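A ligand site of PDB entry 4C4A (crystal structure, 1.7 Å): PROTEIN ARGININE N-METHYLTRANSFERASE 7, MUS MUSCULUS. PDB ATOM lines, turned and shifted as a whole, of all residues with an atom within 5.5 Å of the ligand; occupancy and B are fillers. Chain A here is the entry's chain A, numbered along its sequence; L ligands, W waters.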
ATOM      1  N   TYR A  35      29.338 -34.149 -11.480  1.00  0.00           N
ATOM      2  CA  TYR A  35      28.231 -34.692 -10.695  1.00  0.00           C
ATOM      3  C   TYR A  35      27.885 -36.142 -11.046  1.00  0.00           C
ATOM      4  O   TYR A  35      27.604 -36.943 -10.160  1.00  0.00           O
ATOM      5  CB  TYR A  35      26.984 -33.807 -10.854  1.00  0.00           C
ATOM      6  CG  TYR A  35      27.211 -32.415 -10.334  1.00  0.00           C
ATOM      7  CD1 TYR A  35      27.389 -32.185  -8.981  1.00  0.00           C
ATOM      8  CD2 TYR A  35      27.238 -31.330 -11.197  1.00  0.00           C
ATOM      9  CE1 TYR A  35      27.601 -30.897  -8.489  1.00  0.00           C
ATOM     10  CE2 TYR A  35      27.438 -30.047 -10.718  1.00  0.00           C
ATOM     11  CZ  TYR A  35      27.629 -29.834  -9.362  1.00  0.00           C
ATOM     12  OH  TYR A  35      27.826 -28.560  -8.893  1.00  0.00           O
ATOM     13  N   MET A  38      30.387 -38.543  -9.502  1.00  0.00           N
ATOM     14  CA  MET A  38      30.173 -38.690  -8.062  1.00  0.00           C
ATOM     15  C   MET A  38      29.085 -39.708  -7.796  1.00  0.00           C
ATOM     16  O   MET A  38      29.251 -40.598  -6.966  1.00  0.00           O
ATOM     17  CB  MET A  38      29.789 -37.342  -7.430  1.00  0.00           C
ATOM     18  CG  MET A  38      30.858 -36.274  -7.539  1.00  0.00           C
ATOM     19  SD  MET A  38      30.321 -34.730  -6.789  1.00  0.00           S
ATOM     20  CE  MET A  38      31.049 -33.552  -7.917  1.00  0.00           C
ATOM     21  N   LEU A  39      27.976 -39.614  -8.530  1.00  0.00           N
ATOM     22  CA  LEU A  39      26.834 -40.494  -8.264  1.00  0.00           C
ATOM     23  C   LEU A  39      27.199 -41.943  -8.533  1.00  0.00           C
ATOM     24  O   LEU A  39      26.667 -42.859  -7.893  1.00  0.00           O
ATOM     25  CB  LEU A  39      25.620 -40.076  -9.100  1.00  0.00           C
ATOM     26  CG  LEU A  39      24.989 -38.731  -8.748  1.00  0.00           C
ATOM     27  CD1 LEU A  39      23.895 -38.368  -9.770  1.00  0.00           C
ATOM     28  CD2 LEU A  39      24.420 -38.734  -7.323  1.00  0.00           C
ATOM     29  N   ARG A  44      32.627 -43.969  -2.444  1.00  0.00           N
ATOM     30  CA  ARG A  44      32.309 -42.676  -1.833  1.00  0.00           C
ATOM     31  C   ARG A  44      30.920 -42.649  -1.187  1.00  0.00           C
ATOM     32  O   ARG A  44      30.739 -42.201  -0.043  1.00  0.00           O
ATOM     33  CB  ARG A  44      32.391 -41.569  -2.872  1.00  0.00           C
ATOM     34  CG  ARG A  44      32.147 -40.166  -2.315  1.00  0.00           C
ATOM     35  CD  ARG A  44      31.926 -39.195  -3.456  1.00  0.00           C
ATOM     36  NE  ARG A  44      30.486 -39.050  -3.696  1.00  0.00           N
ATOM     37  CZ  ARG A  44      29.846 -37.893  -3.662  1.00  0.00           C
ATOM     38  NH1 ARG A  44      30.533 -36.766  -3.454  1.00  0.00           N
ATOM     39  NH2 ARG A  44      28.542 -37.851  -3.863  1.00  0.00           N
ATOM     40  N   ASP A  70      24.860 -29.072   5.523  1.00  0.00           N
ATOM     41  CA  ASP A  70      25.480 -29.785   4.406  1.00  0.00           C
ATOM     42  C   ASP A  70      26.039 -28.739   3.454  1.00  0.00           C
ATOM     43  O   ASP A  70      25.274 -28.146   2.705  1.00  0.00           O
ATOM     44  CB  ASP A  70      24.419 -30.678   3.726  1.00  0.00           C
ATOM     45  CG  ASP A  70      24.916 -31.359   2.463  1.00  0.00           C
ATOM     46  OD1 ASP A  70      26.114 -31.277   2.145  1.00  0.00           O
ATOM     47  OD2 ASP A  70      24.059 -32.042   1.820  1.00  0.00           O
ATOM     48  N   ILE A  71      27.347 -28.477   3.506  1.00  0.00           N
ATOM     49  CA  ILE A  71      27.937 -27.429   2.678  1.00  0.00           C
ATOM     50  C   ILE A  71      28.323 -27.973   1.318  1.00  0.00           C
ATOM     51  O   ILE A  71      29.176 -28.855   1.220  1.00  0.00           O
ATOM     52  CB  ILE A  71      29.161 -26.796   3.344  1.00  0.00           C
ATOM     53  CG1 ILE A  71      28.763 -26.290   4.724  1.00  0.00           C
ATOM     54  CG2 ILE A  71      29.733 -25.658   2.472  1.00  0.00           C
ATOM     55  CD1 ILE A  71      29.891 -25.623   5.480  1.00  0.00           C
ATOM     56  N   GLY A  72      27.713 -27.415   0.276  1.00  0.00           N
ATOM     57  CA  GLY A  72      27.974 -27.830  -1.092  1.00  0.00           C
ATOM     58  C   GLY A  72      27.138 -29.046  -1.446  1.00  0.00           C
ATOM     59  O   GLY A  72      27.664 -30.092  -1.829  1.00  0.00           O
ATOM     60  N   THR A  73      25.815 -28.892  -1.340  1.00  0.00           N
ATOM     61  CA  THR A  73      24.937 -30.052  -1.328  1.00  0.00           C
ATOM     62  C   THR A  73      24.784 -30.730  -2.696  1.00  0.00           C
ATOM     63  O   THR A  73      24.432 -31.917  -2.763  1.00  0.00           O
ATOM     64  CB  THR A  73      23.544 -29.675  -0.764  1.00  0.00           C
ATOM     65  OG1 THR A  73      22.841 -30.856  -0.358  1.00  0.00           O
ATOM     66  CG2 THR A  73      22.714 -28.896  -1.777  1.00  0.00           C
ATOM     67  N   GLY A  74      25.085 -30.033  -3.789  1.00  0.00           N
ATOM     68  CA  GLY A  74      24.939 -30.638  -5.107  1.00  0.00           C
ATOM     69  C   GLY A  74      23.511 -31.125  -5.368  1.00  0.00           C
ATOM     70  O   GLY A  74      22.566 -30.340  -5.378  1.00  0.00           O
ATOM     71  N   THR A  75      23.357 -32.440  -5.550  1.00  0.00           N
ATOM     72  CA  THR A  75      22.040 -33.051  -5.754  1.00  0.00           C
ATOM     73  C   THR A  75      21.150 -33.045  -4.517  1.00  0.00           C
ATOM     74  O   THR A  75      19.937 -33.264  -4.610  1.00  0.00           O
ATOM     75  CB  THR A  75      22.185 -34.509  -6.189  1.00  0.00           C
ATOM     76  OG1 THR A  75      22.902 -35.220  -5.180  1.00  0.00           O
ATOM     77  CG2 THR A  75      22.923 -34.615  -7.521  1.00  0.00           C
ATOM     78  N   LEU A  77      22.024 -35.271  -2.158  1.00  0.00           N
ATOM     79  CA  LEU A  77      22.222 -36.669  -1.723  1.00  0.00           C
ATOM     80  C   LEU A  77      22.551 -36.843  -0.230  1.00  0.00           C
ATOM     81  O   LEU A  77      21.899 -37.622   0.472  1.00  0.00           O
ATOM     82  CB  LEU A  77      23.336 -37.335  -2.553  1.00  0.00           C
ATOM     83  CG  LEU A  77      23.603 -38.808  -2.249  1.00  0.00           C
ATOM     84  CD1 LEU A  77      22.413 -39.644  -2.664  1.00  0.00           C
ATOM     85  CD2 LEU A  77      24.868 -39.297  -2.955  1.00  0.00           C
ATOM     86  N   LEU A  78      23.560 -36.120   0.268  1.00  0.00           N
ATOM     87  CA  LEU A  78      24.029 -36.360   1.628  1.00  0.00           C
ATOM     88  C   LEU A  78      22.993 -35.894   2.653  1.00  0.00           C
ATOM     89  O   LEU A  78      22.875 -36.481   3.724  1.00  0.00           O
ATOM     90  CB  LEU A  78      25.383 -35.690   1.875  1.00  0.00           C
ATOM     91  CG  LEU A  78      26.496 -36.105   0.887  1.00  0.00           C
ATOM     92  CD1 LEU A  78      27.816 -35.433   1.221  1.00  0.00           C
ATOM     93  CD2 LEU A  78      26.687 -37.630   0.801  1.00  0.00           C
ATOM     94  N   ILE A  93      23.410 -26.219   1.519  1.00  0.00           N
ATOM     95  CA  ILE A  93      23.914 -24.989   0.928  1.00  0.00           C
ATOM     96  C   ILE A  93      24.542 -25.297  -0.421  1.00  0.00           C
ATOM     97  O   ILE A  93      25.346 -26.210  -0.524  1.00  0.00           O
ATOM     98  CB  ILE A  93      24.970 -24.290   1.835  1.00  0.00           C
ATOM     99  CG1 ILE A  93      24.601 -24.373   3.325  1.00  0.00           C
ATOM    100  CG2 ILE A  93      25.190 -22.822   1.405  1.00  0.00           C
ATOM    101  CD1 ILE A  93      23.230 -23.799   3.695  1.00  0.00           C
ATOM    102  N   GLU A  94      24.173 -24.547  -1.452  1.00  0.00           N
ATOM    103  CA  GLU A  94      24.746 -24.760  -2.790  1.00  0.00           C
ATOM    104  C   GLU A  94      24.883 -23.443  -3.516  1.00  0.00           C
ATOM    105  O   GLU A  94      23.890 -22.783  -3.810  1.00  0.00           O
ATOM    106  CB  GLU A  94      23.882 -25.725  -3.607  1.00  0.00           C
ATOM    107  CG  GLU A  94      24.332 -25.875  -5.061  1.00  0.00           C
ATOM    108  CD  GLU A  94      25.789 -26.330  -5.203  1.00  0.00           C
ATOM    109  OE1 GLU A  94      26.141 -27.436  -4.728  1.00  0.00           O
ATOM    110  OE2 GLU A  94      26.601 -25.578  -5.765  1.00  0.00           O
ATOM    111  N   VAL A  95      26.116 -23.066  -3.828  1.00  0.00           N
ATOM    112  CA  VAL A  95      26.373 -21.769  -4.430  1.00  0.00           C
ATOM    113  C   VAL A  95      25.949 -21.715  -5.910  1.00  0.00           C
ATOM    114  O   VAL A  95      25.578 -20.655  -6.406  1.00  0.00           O
ATOM    115  CB  VAL A  95      27.866 -21.389  -4.299  1.00  0.00           C
ATOM    116  CG1 VAL A  95      28.755 -22.357  -5.096  1.00  0.00           C
ATOM    117  CG2 VAL A  95      28.117 -19.947  -4.735  1.00  0.00           C
ATOM    118  N   PHE A  96      25.991 -22.857  -6.588  1.00  0.00           N
ATOM    119  CA  PHE A  96      25.742 -22.893  -8.025  1.00  0.00           C
ATOM    120  C   PHE A  96      24.234 -22.982  -8.297  1.00  0.00           C
ATOM    121  O   PHE A  96      23.596 -23.991  -7.989  1.00  0.00           O
ATOM    122  CB  PHE A  96      26.516 -24.066  -8.638  1.00  0.00           C
ATOM    123  CG  PHE A  96      26.465 -24.131 -10.152  1.00  0.00           C
ATOM    124  CD1 PHE A  96      26.680 -23.009 -10.935  1.00  0.00           C
ATOM    125  CD2 PHE A  96      26.242 -25.343 -10.788  1.00  0.00           C
ATOM    126  CE1 PHE A  96      26.645 -23.074 -12.317  1.00  0.00           C
ATOM    127  CE2 PHE A  96      26.213 -25.423 -12.189  1.00  0.00           C
ATOM    128  CZ  PHE A  96      26.416 -24.295 -12.943  1.00  0.00           C
ATOM    129  N   MET A  99      22.268 -25.991  -9.857  1.00  0.00           N
ATOM    130  CA  MET A  99      22.310 -27.199  -9.042  1.00  0.00           C
ATOM    131  C   MET A  99      21.459 -27.045  -7.785  1.00  0.00           C
ATOM    132  O   MET A  99      20.853 -28.019  -7.323  1.00  0.00           O
ATOM    133  CB  MET A  99      23.759 -27.541  -8.684  1.00  0.00           C
ATOM    134  CG  MET A  99      24.495 -28.233  -9.829  1.00  0.00           C
ATOM    135  SD  MET A  99      23.693 -29.788 -10.289  1.00  0.00           S
ATOM    136  CE  MET A  99      24.021 -30.699  -8.786  1.00  0.00           C
ATOM    137  N   LYS A 121      23.363 -20.015  -1.865  1.00  0.00           N
ATOM    138  CA  LYS A 121      24.354 -19.035  -1.447  1.00  0.00           C
ATOM    139  C   LYS A 121      25.695 -19.764  -1.323  1.00  0.00           C
ATOM    140  O   LYS A 121      25.739 -20.987  -1.192  1.00  0.00           O
ATOM    141  CB  LYS A 121      23.977 -18.405  -0.089  1.00  0.00           C
ATOM    142  CG  LYS A 121      22.733 -17.538  -0.085  1.00  0.00           C
ATOM    143  CD  LYS A 121      22.511 -16.908   1.301  1.00  0.00           C
ATOM    144  CE  LYS A 121      21.307 -15.983   1.308  1.00  0.00           C
ATOM    145  NZ  LYS A 121      21.099 -15.359   2.646  1.00  0.00           N
ATOM    146  N   HIS A 122      26.790 -19.003  -1.339  1.00  0.00           N
ATOM    147  CA  HIS A 122      28.052 -19.524  -0.837  1.00  0.00           C
ATOM    148  C   HIS A 122      27.935 -19.610   0.693  1.00  0.00           C
ATOM    149  O   HIS A 122      27.360 -18.715   1.306  1.00  0.00           O
ATOM    150  CB  HIS A 122      29.214 -18.617  -1.243  1.00  0.00           C
ATOM    151  CG  HIS A 122      30.566 -19.252  -1.090  1.00  0.00           C
ATOM    152  ND1 HIS A 122      31.316 -19.123   0.060  1.00  0.00           N
ATOM    153  CD2 HIS A 122      31.299 -20.007  -1.940  1.00  0.00           C
ATOM    154  CE1 HIS A 122      32.459 -19.779  -0.092  1.00  0.00           C
ATOM    155  NE2 HIS A 122      32.467 -20.318  -1.294  1.00  0.00           N
ATOM    156  N   SER A 123      28.478 -20.660   1.299  1.00  0.00           N
ATOM    157  CA  SER A 123      28.321 -20.846   2.746  1.00  0.00           C
ATOM    158  C   SER A 123      28.890 -19.667   3.543  1.00  0.00           C
ATOM    159  O   SER A 123      28.421 -19.375   4.649  1.00  0.00           O
ATOM    160  CB  SER A 123      28.970 -22.146   3.210  1.00  0.00           C
ATOM    161  OG  SER A 123      30.375 -22.127   3.049  1.00  0.00           O
ATOM    162  N   THR A 124      29.884 -18.973   3.003  1.00  0.00           N
ATOM    163  CA  THR A 124      30.460 -17.840   3.742  1.00  0.00           C
ATOM    164  C   THR A 124      29.508 -16.628   3.789  1.00  0.00           C
ATOM    165  O   THR A 124      29.766 -15.660   4.516  1.00  0.00           O
ATOM    166  CB  THR A 124      31.815 -17.404   3.150  1.00  0.00           C
ATOM    167  OG1 THR A 124      31.642 -16.999   1.790  1.00  0.00           O
ATOM    168  CG2 THR A 124      32.830 -18.550   3.219  1.00  0.00           C
ATOM    169  N   THR A 143      30.218 -32.180   4.627  1.00  0.00           N
ATOM    170  CA  THR A 143      30.627 -31.532   3.376  1.00  0.00           C
ATOM    171  C   THR A 143      31.328 -32.504   2.457  1.00  0.00           C
ATOM    172  O   THR A 143      31.952 -33.477   2.909  1.00  0.00           O
ATOM    173  CB  THR A 143      31.599 -30.312   3.574  1.00  0.00           C
ATOM    174  OG1 THR A 143      32.965 -30.710   3.400  1.00  0.00           O
ATOM    175  CG2 THR A 143      31.428 -29.629   4.935  1.00  0.00           C
ATOM    176  N   GLU A 144      31.248 -32.236   1.152  1.00  0.00           N
ATOM    177  CA  GLU A 144      32.134 -32.874   0.184  1.00  0.00           C
ATOM    178  C   GLU A 144      32.745 -31.768  -0.674  1.00  0.00           C
ATOM    179  O   GLU A 144      32.392 -31.603  -1.836  1.00  0.00           O
ATOM    180  CB  GLU A 144      31.377 -33.903  -0.669  1.00  0.00           C
ATOM    181  CG  GLU A 144      32.289 -35.000  -1.268  1.00  0.00           C
ATOM    182  CD  GLU A 144      33.077 -34.531  -2.490  1.00  0.00           C
ATOM    183  OE1 GLU A 144      34.026 -33.724  -2.333  1.00  0.00           O
ATOM    184  OE2 GLU A 144      32.765 -35.014  -3.610  1.00  0.00           O
ATOM    185  N   LEU A 145      33.644 -30.993  -0.079  1.00  0.00           N
ATOM    186  CA  LEU A 145      34.209 -29.814  -0.732  1.00  0.00           C
ATOM    187  C   LEU A 145      35.607 -30.071  -1.299  1.00  0.00           C
ATOM    188  O   LEU A 145      36.345 -29.133  -1.614  1.00  0.00           O
ATOM    189  CB  LEU A 145      34.282 -28.649   0.270  1.00  0.00           C
ATOM    190  CG  LEU A 145      32.909 -28.180   0.774  1.00  0.00           C
ATOM    191  CD1 LEU A 145      33.094 -27.186   1.905  1.00  0.00           C
ATOM    192  CD2 LEU A 145      32.124 -27.575  -0.381  1.00  0.00           C
ATOM    193  N   GLU A 153      39.704 -26.403  -3.642  1.00  0.00           N
ATOM    194  CA  GLU A 153      38.412 -25.772  -3.919  1.00  0.00           C
ATOM    195  C   GLU A 153      37.794 -25.176  -2.658  1.00  0.00           C
ATOM    196  O   GLU A 153      36.576 -25.062  -2.549  1.00  0.00           O
ATOM    197  CB  GLU A 153      37.479 -26.773  -4.602  1.00  0.00           C
ATOM    198  CG  GLU A 153      37.977 -27.070  -6.037  1.00  0.00           C
ATOM    199  CD  GLU A 153      37.159 -28.104  -6.786  1.00  0.00           C
ATOM    200  OE1 GLU A 153      36.319 -28.787  -6.168  1.00  0.00           O
ATOM    201  OE2 GLU A 153      37.381 -28.247  -8.015  1.00  0.00           O
ATOM    202  N   SER A 158      36.140 -22.516   3.934  1.00  0.00           N
ATOM    203  CA  SER A 158      34.723 -22.864   4.123  1.00  0.00           C
ATOM    204  C   SER A 158      34.528 -23.478   5.508  1.00  0.00           C
ATOM    205  O   SER A 158      33.600 -23.102   6.217  1.00  0.00           O
ATOM    206  CB  SER A 158      34.228 -23.816   3.026  1.00  0.00           C
ATOM    207  OG  SER A 158      34.122 -23.135   1.786  1.00  0.00           O
HETATM  208  N1  LIG L   1      27.575 -32.852  -1.509  1.00  0.00           N
HETATM  209  C1  LIG L   1      27.288 -33.239  -2.890  1.00  0.00           C
HETATM  210  C2  LIG L   1      28.020 -32.421  -3.977  1.00  0.00           C
HETATM  211  C3  LIG L   1      29.522 -32.317  -3.767  1.00  0.00           C
HETATM  212  S1  LIG L   1      30.339 -31.377  -5.120  1.00  0.00           S
HETATM  213  C4  LIG L   1      27.626 -34.691  -2.961  1.00  0.00           C
HETATM  214  O1  LIG L   1      28.575 -35.128  -2.326  1.00  0.00           O
HETATM  215  O2  LIG L   1      26.829 -35.457  -3.705  1.00  0.00           O
HETATM  216  C5  LIG L   1      30.652 -29.780  -4.294  1.00  0.00           C
HETATM  217  C6  LIG L   1      29.474 -28.808  -4.386  1.00  0.00           C
HETATM  218  O3  LIG L   1      29.750 -27.697  -3.500  1.00  0.00           O
HETATM  219  C7  LIG L   1      29.379 -28.172  -5.795  1.00  0.00           C
HETATM  220  O4  LIG L   1      28.033 -28.291  -6.309  1.00  0.00           O
HETATM  221  C8  LIG L   1      29.850 -26.692  -5.592  1.00  0.00           C
HETATM  222  O5  LIG L   1      29.139 -25.765  -6.425  1.00  0.00           O
HETATM  223  C9  LIG L   1      29.427 -26.421  -4.148  1.00  0.00           C
HETATM  224  N2  LIG L   1      30.231 -25.585  -3.274  1.00  0.00           N
HETATM  225  C10 LIG L   1      31.589 -25.609  -3.066  1.00  0.00           C
HETATM  226  N3  LIG L   1      31.889 -24.804  -2.078  1.00  0.00           N
HETATM  227  C11 LIG L   1      30.729 -24.272  -1.582  1.00  0.00           C
HETATM  228  C12 LIG L   1      30.404 -23.379  -0.557  1.00  0.00           C
HETATM  229  N4  LIG L   1      31.411 -22.854   0.228  1.00  0.00           N
HETATM  230  N5  LIG L   1      29.128 -23.083  -0.350  1.00  0.00           N
HETATM  231  C13 LIG L   1      28.150 -23.580  -1.083  1.00  0.00           C
HETATM  232  N6  LIG L   1      28.403 -24.427  -2.067  1.00  0.00           N
HETATM  233  C14 LIG L   1      29.668 -24.783  -2.334  1.00  0.00           C
HETATM  234  O   HOH W   1      25.454 -34.496  -5.452  1.00  0.00           O
HETATM  235  O   HOH W   2      28.310 -31.772   0.670  1.00  0.00           O
HETATM  236  O   HOH W   3      24.766 -33.524  -0.523  1.00  0.00           O
HETATM  237  O   HOH W   4      30.876 -23.852  -7.448  1.00  0.00           O
HETATM  238  O   HOH W   5      34.537 -24.306  -0.831  1.00  0.00           O
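SD of Met 38 sits close to S1 of the ligand (3.7 Å). Residues that only touch the ligand: Thr 73 (3.1 Å), Leu 145 (3.3 Å), Glu 144 (3.5 Å), Lys 121 (3.5 Å), Leu 78 (3.6 Å), Gly 74 (3.7 Å), Phe 96 (3.8 Å), Ile 71 (3.8 Å) and Ile 93 (3.9 Å). 18 residues have an atom within 4 Å of the ligand: Tyr 35, Met 38, Arg 44, Ile 71, Gly 72, Thr 73, Gly 74, Leu 78, Ile 93, Glu 94, Val 95, Phe 96, Lys 121, His 122, Ser 123, Glu 144, Leu 145 and Ser 158.
Water W1 bridges an oxygen (O2) of the ligand and the side-chain hydroxyl of Thr 75. Water W5 lies within hydrogen-bond range of O of Glu 153, OG of Ser 158 and N3 of the ligand. Water W3 lies within hydrogen-bond range of the backbone carbonyl oxygen of Thr 73 (2.8 Å), the side-chain carboxylate of Asp 70 (2.9 Å), the backbone NH of Leu 78 (3.0 Å) and a nitrogen (N1) of the ligand (3.1 Å).
The backbone carbonyl oxygen (O) of Glu 94 is in hydrogen-bond range of the backbone NH (N) of Lys 121 (3.4 Å). OE1 of Glu 94 is in hydrogen-bond range of N of Gly 74, 3.0 Å away. The side-chain carboxylate of Glu 94 lies within hydrogen-bond range of the backbone NH of Phe 96 (2.9 Å). N of Gly 72 lies within hydrogen-bond range of O of Ile 93 (2.8 Å). The backbone carbonyl oxygen of Ile 93 lies within hydrogen-bond range of the backbone NH of Thr 73, at 2.8 Å. The side-chain hydroxyl (OG1) of Thr 73 lies within hydrogen-bond range of the side-chain carboxylate (OD2) of Asp 70 (2.8 Å). O of Lys 121 sits at hydrogen-bond distance from N of Val 95 (3.4 Å). O of Asp 70 sits at hydrogen-bond distance from N of Ile 93 (2.9 Å).
The side-chain hydroxyl (OH) of Tyr 35 is in hydrogen-bond range of an oxygen (O4) of the ligand, at 2.6 Å. An oxygen (O4) of the ligand sits at hydrogen-bond distance from the side-chain carboxylate (OE1) of Glu 94. The backbone carbonyl oxygen (O) of Gly 72 sits at hydrogen-bond distance from a nitrogen (N1) of the ligand (2.8 Å). The guanidinium group of Arg 44 lies within salt-bridge range of an oxygen (O1) of the ligand (2.8 Å). N of Ser 123 is in hydrogen-bond range of N5 of the ligand, at 3.0 Å. N4 of the ligand sits at hydrogen-bond distance from OG of Ser 123 (3.1 Å). A nitrogen (N4) of the ligand is in hydrogen-bond range of the side-chain hydroxyl (OG) of Ser 158. A ring nitrogen (NE2) of His 122 lies within hydrogen-bond range of a nitrogen (N4) of the ligand. A nitrogen (N6) of the ligand lies within hydrogen-bond range of the backbone NH of Val 95 (3.2 Å).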
